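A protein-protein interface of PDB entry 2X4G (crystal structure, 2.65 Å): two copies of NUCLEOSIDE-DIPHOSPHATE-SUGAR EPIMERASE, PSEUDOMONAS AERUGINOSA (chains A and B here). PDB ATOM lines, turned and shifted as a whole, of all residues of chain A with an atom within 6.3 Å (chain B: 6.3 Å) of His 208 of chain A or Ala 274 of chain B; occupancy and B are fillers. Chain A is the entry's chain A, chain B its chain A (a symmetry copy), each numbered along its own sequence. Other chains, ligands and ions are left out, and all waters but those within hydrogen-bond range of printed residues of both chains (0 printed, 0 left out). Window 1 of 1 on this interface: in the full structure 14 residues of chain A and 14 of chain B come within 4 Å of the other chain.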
ATOM      1  N   GLU A 205      20.438  21.495  27.448  1.00  0.00           N
ATOM      2  CA  GLU A 205      20.949  22.223  28.609  1.00  0.00           C
ATOM      3  C   GLU A 205      21.871  23.366  28.206  1.00  0.00           C
ATOM      4  O   GLU A 205      21.705  24.500  28.657  1.00  0.00           O
ATOM      5  CB  GLU A 205      21.686  21.273  29.556  1.00  0.00           C
ATOM      6  CG  GLU A 205      20.784  20.194  30.199  1.00  0.00           C
ATOM      7  CD  GLU A 205      21.332  19.683  31.550  1.00  0.00           C
ATOM      8  OE1 GLU A 205      22.575  19.760  31.763  1.00  0.00           O
ATOM      9  OE2 GLU A 205      20.519  19.226  32.400  1.00  0.00           O
ATOM     10  N   MET A 206      22.860  23.078  27.373  1.00  0.00           N
ATOM     11  CA  MET A 206      23.758  24.133  26.907  1.00  0.00           C
ATOM     12  C   MET A 206      23.062  24.988  25.851  1.00  0.00           C
ATOM     13  O   MET A 206      23.139  24.726  24.654  1.00  0.00           O
ATOM     14  CB  MET A 206      25.049  23.574  26.346  1.00  0.00           C
ATOM     15  CG  MET A 206      26.020  24.657  26.052  1.00  0.00           C
ATOM     16  SD  MET A 206      27.467  24.017  25.258  1.00  0.00           S
ATOM     17  CE  MET A 206      28.545  23.638  26.642  1.00  0.00           C
ATOM     18  N   THR A 207      22.390  26.023  26.323  1.00  0.00           N
ATOM     19  CA  THR A 207      21.641  26.886  25.452  1.00  0.00           C
ATOM     20  C   THR A 207      22.514  28.011  24.897  1.00  0.00           C
ATOM     21  O   THR A 207      22.152  28.635  23.907  1.00  0.00           O
ATOM     22  CB  THR A 207      20.403  27.427  26.176  1.00  0.00           C
ATOM     23  OG1 THR A 207      19.601  28.143  25.243  1.00  0.00           O
ATOM     24  CG2 THR A 207      20.770  28.340  27.357  1.00  0.00           C
ATOM     25  N   HIS A 208      23.665  28.264  25.521  1.00  0.00           N
ATOM     26  CA  HIS A 208      24.591  29.314  25.066  1.00  0.00           C
ATOM     27  C   HIS A 208      26.046  28.868  25.231  1.00  0.00           C
ATOM     28  O   HIS A 208      26.335  27.939  25.989  1.00  0.00           O
ATOM     29  CB  HIS A 208      24.393  30.615  25.873  1.00  0.00           C
ATOM     30  CG  HIS A 208      23.041  31.241  25.725  1.00  0.00           C
ATOM     31  ND1 HIS A 208      22.733  32.118  24.708  1.00  0.00           N
ATOM     32  CD2 HIS A 208      21.923  31.141  26.483  1.00  0.00           C
ATOM     33  CE1 HIS A 208      21.478  32.514  24.833  1.00  0.00           C
ATOM     34  NE2 HIS A 208      20.962  31.934  25.903  1.00  0.00           N
ATOM     35  N   TYR A 209      26.954  29.560  24.540  1.00  0.00           N
ATOM     36  CA  TYR A 209      28.403  29.327  24.649  1.00  0.00           C
ATOM     37  C   TYR A 209      29.112  30.671  24.750  1.00  0.00           C
ATOM     38  O   TYR A 209      28.531  31.703  24.405  1.00  0.00           O
ATOM     39  CB  TYR A 209      28.933  28.607  23.402  1.00  0.00           C
ATOM     40  CG  TYR A 209      28.932  29.494  22.171  1.00  0.00           C
ATOM     41  CD1 TYR A 209      27.789  29.634  21.392  1.00  0.00           C
ATOM     42  CD2 TYR A 209      30.062  30.213  21.803  1.00  0.00           C
ATOM     43  CE1 TYR A 209      27.778  30.451  20.261  1.00  0.00           C
ATOM     44  CE2 TYR A 209      30.057  31.049  20.670  1.00  0.00           C
ATOM     45  CZ  TYR A 209      28.906  31.162  19.906  1.00  0.00           C
ATOM     46  OH  TYR A 209      28.862  31.987  18.791  1.00  0.00           O
ATOM     47  N   VAL A 210      30.371  30.650  25.183  1.00  0.00           N
ATOM     48  CA  VAL A 210      31.209  31.843  25.232  1.00  0.00           C
ATOM     49  C   VAL A 210      32.343  31.760  24.206  1.00  0.00           C
ATOM     50  O   VAL A 210      33.033  30.748  24.119  1.00  0.00           O
ATOM     51  CB  VAL A 210      31.805  32.039  26.644  1.00  0.00           C
ATOM     52  CG1 VAL A 210      33.010  32.976  26.609  1.00  0.00           C
ATOM     53  CG2 VAL A 210      30.747  32.590  27.583  1.00  0.00           C
ATOM     54  N   THR A 252      30.374  24.150  18.855  1.00  0.00           N
ATOM     55  CA  THR A 252      29.013  24.228  19.315  1.00  0.00           C
ATOM     56  C   THR A 252      28.067  23.926  18.189  1.00  0.00           C
ATOM     57  O   THR A 252      27.104  23.184  18.355  1.00  0.00           O
ATOM     58  CB  THR A 252      28.758  25.647  19.832  1.00  0.00           C
ATOM     59  OG1 THR A 252      28.974  25.641  21.237  1.00  0.00           O
ATOM     60  CG2 THR A 252      27.354  26.167  19.505  1.00  0.00           C
ATOM     61  N   PRO A 264      23.590  26.649  19.881  1.00  0.00           N
ATOM     62  CA  PRO A 264      23.722  27.544  21.013  1.00  0.00           C
ATOM     63  C   PRO A 264      24.151  28.933  20.588  1.00  0.00           C
ATOM     64  O   PRO A 264      24.992  29.084  19.716  1.00  0.00           O
ATOM     65  CB  PRO A 264      24.822  26.893  21.846  1.00  0.00           C
ATOM     66  CG  PRO A 264      24.722  25.468  21.562  1.00  0.00           C
ATOM     67  CD  PRO A 264      24.175  25.326  20.168  1.00  0.00           C
ATOM     68  N   GLN A 265      23.573  29.931  21.236  1.00  0.00           N
ATOM     69  CA  GLN A 265      23.800  31.312  20.880  1.00  0.00           C
ATOM     70  C   GLN A 265      24.981  31.877  21.650  1.00  0.00           C
ATOM     71  O   GLN A 265      25.290  31.414  22.744  1.00  0.00           O
ATOM     72  CB  GLN A 265      22.534  32.140  21.141  1.00  0.00           C
ATOM     73  CG  GLN A 265      21.231  31.558  20.534  1.00  0.00           C
ATOM     74  CD  GLN A 265      21.259  31.401  18.992  1.00  0.00           C
ATOM     75  OE1 GLN A 265      22.307  31.532  18.338  1.00  0.00           O
ATOM     76  NE2 GLN A 265      20.088  31.116  18.413  1.00  0.00           N
ATOM     77  N   PRO A 266      25.655  32.882  21.068  1.00  0.00           N
ATOM     78  CA  PRO A 266      26.825  33.432  21.721  1.00  0.00           C
ATOM     79  C   PRO A 266      26.435  34.188  22.954  1.00  0.00           C
ATOM     80  O   PRO A 266      25.352  34.755  23.022  1.00  0.00           O
ATOM     81  CB  PRO A 266      27.416  34.404  20.688  1.00  0.00           C
ATOM     82  CG  PRO A 266      26.517  34.389  19.525  1.00  0.00           C
ATOM     83  CD  PRO A 266      25.264  33.675  19.893  1.00  0.00           C
ATOM     84  N   MET A 267      27.324  34.184  23.925  1.00  0.00           N
ATOM     85  CA  MET A 267      27.112  34.922  25.125  1.00  0.00           C
ATOM     86  C   MET A 267      28.355  35.734  25.375  1.00  0.00           C
ATOM     87  O   MET A 267      29.462  35.208  25.344  1.00  0.00           O
ATOM     88  CB  MET A 267      26.861  33.967  26.267  1.00  0.00           C
ATOM     89  CG  MET A 267      26.289  34.641  27.482  1.00  0.00           C
ATOM     90  SD  MET A 267      26.181  33.467  28.822  1.00  0.00           S
ATOM     91  CE  MET A 267      27.933  33.197  29.100  1.00  0.00           C
ATOM     92  N   SER B 268      19.120  37.925  30.446  1.00  0.00           N
ATOM     93  CA  SER B 268      18.106  36.875  30.394  1.00  0.00           C
ATOM     94  C   SER B 268      18.257  35.869  31.534  1.00  0.00           C
ATOM     95  O   SER B 268      19.349  35.651  32.054  1.00  0.00           O
ATOM     96  CB  SER B 268      18.185  36.153  29.041  1.00  0.00           C
ATOM     97  OG  SER B 268      17.366  35.009  29.014  1.00  0.00           O
ATOM     98  N   MET B 269      17.143  35.273  31.926  1.00  0.00           N
ATOM     99  CA  MET B 269      17.160  34.241  32.938  1.00  0.00           C
ATOM    100  C   MET B 269      17.794  32.975  32.382  1.00  0.00           C
ATOM    101  O   MET B 269      18.554  32.297  33.075  1.00  0.00           O
ATOM    102  CB  MET B 269      15.739  33.932  33.403  1.00  0.00           C
ATOM    103  CG  MET B 269      15.685  33.000  34.612  1.00  0.00           C
ATOM    104  SD  MET B 269      16.574  33.692  36.008  1.00  0.00           S
ATOM    105  CE  MET B 269      15.548  35.149  36.274  1.00  0.00           C
ATOM    106  N   ALA B 270      17.466  32.664  31.133  1.00  0.00           N
ATOM    107  CA  ALA B 270      18.071  31.543  30.424  1.00  0.00           C
ATOM    108  C   ALA B 270      19.591  31.700  30.300  1.00  0.00           C
ATOM    109  O   ALA B 270      20.337  30.713  30.388  1.00  0.00           O
ATOM    110  CB  ALA B 270      17.443  31.396  29.044  1.00  0.00           C
ATOM    111  N   MET B 271      20.044  32.941  30.113  1.00  0.00           N
ATOM    112  CA  MET B 271      21.465  33.230  29.957  1.00  0.00           C
ATOM    113  C   MET B 271      22.198  33.101  31.276  1.00  0.00           C
ATOM    114  O   MET B 271      23.411  32.976  31.289  1.00  0.00           O
ATOM    115  CB  MET B 271      21.663  34.632  29.399  1.00  0.00           C
ATOM    116  CG  MET B 271      22.791  34.752  28.390  1.00  0.00           C
ATOM    117  SD  MET B 271      22.394  35.989  27.119  1.00  0.00           S
ATOM    118  CE  MET B 271      23.468  35.546  25.744  1.00  0.00           C
ATOM    119  N   ALA B 272      21.455  33.145  32.380  1.00  0.00           N
ATOM    120  CA  ALA B 272      21.998  32.918  33.719  1.00  0.00           C
ATOM    121  C   ALA B 272      22.209  31.437  33.982  1.00  0.00           C
ATOM    122  O   ALA B 272      23.256  31.033  34.479  1.00  0.00           O
ATOM    123  CB  ALA B 272      21.078  33.513  34.772  1.00  0.00           C
ATOM    124  N   ARG B 273      21.209  30.628  33.650  1.00  0.00           N
ATOM    125  CA  ARG B 273      21.336  29.164  33.760  1.00  0.00           C
ATOM    126  C   ARG B 273      22.372  28.594  32.801  1.00  0.00           C
ATOM    127  O   ARG B 273      23.079  27.644  33.141  1.00  0.00           O
ATOM    128  CB  ARG B 273      19.992  28.477  33.519  1.00  0.00           C
ATOM    129  CG  ARG B 273      19.077  28.526  34.722  1.00  0.00           C
ATOM    130  CD  ARG B 273      17.612  28.458  34.331  1.00  0.00           C
ATOM    131  NE  ARG B 273      16.769  28.855  35.459  1.00  0.00           N
ATOM    132  CZ  ARG B 273      15.470  29.146  35.378  1.00  0.00           C
ATOM    133  NH1 ARG B 273      14.826  29.085  34.209  1.00  0.00           N
ATOM    134  NH2 ARG B 273      14.813  29.503  36.477  1.00  0.00           N
ATOM    135  N   ALA B 274      22.449  29.174  31.604  1.00  0.00           N
ATOM    136  CA  ALA B 274      23.434  28.761  30.608  1.00  0.00           C
ATOM    137  C   ALA B 274      24.880  28.984  31.075  1.00  0.00           C
ATOM    138  O   ALA B 274      25.784  28.311  30.586  1.00  0.00           O
ATOM    139  CB  ALA B 274      23.187  29.464  29.284  1.00  0.00           C
ATOM    140  N   LEU B 275      25.097  29.915  32.006  1.00  0.00           N
ATOM    141  CA  LEU B 275      26.409  30.091  32.638  1.00  0.00           C
ATOM    142  C   LEU B 275      26.603  29.096  33.759  1.00  0.00           C
ATOM    143  O   LEU B 275      27.669  28.505  33.893  1.00  0.00           O
ATOM    144  CB  LEU B 275      26.591  31.514  33.182  1.00  0.00           C
ATOM    145  CG  LEU B 275      27.136  32.499  32.143  1.00  0.00           C
ATOM    146  CD1 LEU B 275      27.167  33.916  32.645  1.00  0.00           C
ATOM    147  CD2 LEU B 275      28.542  32.085  31.720  1.00  0.00           C
ATOM    148  N   ALA B 276      25.569  28.915  34.572  1.00  0.00           N
ATOM    149  CA  ALA B 276      25.580  27.874  35.581  1.00  0.00           C
ATOM    150  C   ALA B 276      25.946  26.519  34.953  1.00  0.00           C
ATOM    151  O   ALA B 276      26.674  25.728  35.557  1.00  0.00           O
ATOM    152  CB  ALA B 276      24.238  27.804  36.250  1.00  0.00           C
ATOM    153  N   THR B 277      25.451  26.284  33.736  1.00  0.00           N
ATOM    154  CA  THR B 277      25.671  25.041  32.978  1.00  0.00           C
ATOM    155  C   THR B 277      27.080  24.929  32.381  1.00  0.00           C
ATOM    156  O   THR B 277      27.659  23.838  32.331  1.00  0.00           O
ATOM    157  CB  THR B 277      24.627  24.915  31.824  1.00  0.00           C
ATOM    158  OG1 THR B 277      23.300  24.915  32.374  1.00  0.00           O
ATOM    159  CG2 THR B 277      24.840  23.651  30.995  1.00  0.00           C
ATOM    160  N   LEU B 278      27.617  26.045  31.899  1.00  0.00           N
ATOM    161  CA  LEU B 278      29.021  26.091  31.486  1.00  0.00           C
ATOM    162  C   LEU B 278      29.943  25.834  32.689  1.00  0.00           C
ATOM    163  O   LEU B 278      31.002  25.215  32.541  1.00  0.00           O
ATOM    164  CB  LEU B 278      29.356  27.434  30.826  1.00  0.00           C
ATOM    165  CG  LEU B 278      29.101  27.549  29.318  1.00  0.00           C
ATOM    166  CD1 LEU B 278      27.684  27.134  28.941  1.00  0.00           C
ATOM    167  CD2 LEU B 278      29.399  28.971  28.841  1.00  0.00           C
ATOM    168  N   GLY B 279      29.531  26.310  33.868  1.00  0.00           N
ATOM    169  CA  GLY B 279      30.220  26.007  35.122  1.00  0.00           C
ATOM    170  C   GLY B 279      30.417  24.514  35.338  1.00  0.00           C
ATOM    171  O   GLY B 279      31.541  24.061  35.548  1.00  0.00           O
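SD of Met 267 of chain A sits close to O of Met 271 of chain B (3.7 Å).
The backbone carbonyl oxygen (O) of Thr 207 of chain A is in hydrogen-bond range of the backbone NH (N) of Gln 265 of chain A, at 3.3 Å.
A ring nitrogen (ND1) of His 208 of chain A sits close to the backbone carbonyl oxygen of Gln 265 of chain A (3.3 Å).
The backbone carbonyl oxygen (O) of Tyr 209 of chain A sits at hydrogen-bond distance from the backbone NH (N) of Met 267 of chain A (2.8 Å).
The side-chain hydroxyl (OG) of Ser 268 of chain B is in hydrogen-bond range of the backbone NH (N) of Ala 270 of chain B, 3.2 Å away.
Among the printed residues, merely in contact across the chains: Met 267 of chain A with Leu 275 of chain B, Thr 207 of chain A with Ala 274 of chain B, His 208 of chain A with Leu 278 of chain B, Pro 266 of chain A with Met 271 of chain B, His 208 of chain A with Ala 274 of chain B, His 208 of chain A with Met 271 of chain B and Thr 207 of chain A with Ala 270 of chain B.
Of the printed residues of chain A, Leu 275 of chain B touches Met 267 (2.9 Å).
Of the printed residues of chain A, Leu 278 of chain B touches His 208.
Of the printed residues of chain A, Met 271 of chain B touches His 208, Pro 266 and Met 267.
Of the printed residues of chain A, Ala 270 of chain B touches Thr 207.
Ser 268 of chain B touches none of the printed residues of chain A.
Hydrophobic or aromatic side chains of chain A that line the printed part of chain B: His 208 and Met 267.
Of the 12 printed residues of chain B, 5 touch a printed residue of chain A.
Hydrophobic or aromatic side chains of chain B that line the printed part of chain A: Met 271, Ala 274, Leu 275 and Leu 278.
No position is printed for both chains.
Of the 8 pairs that touch across the chains among the printed residues, none has its exchanged pair printed and touching as well.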
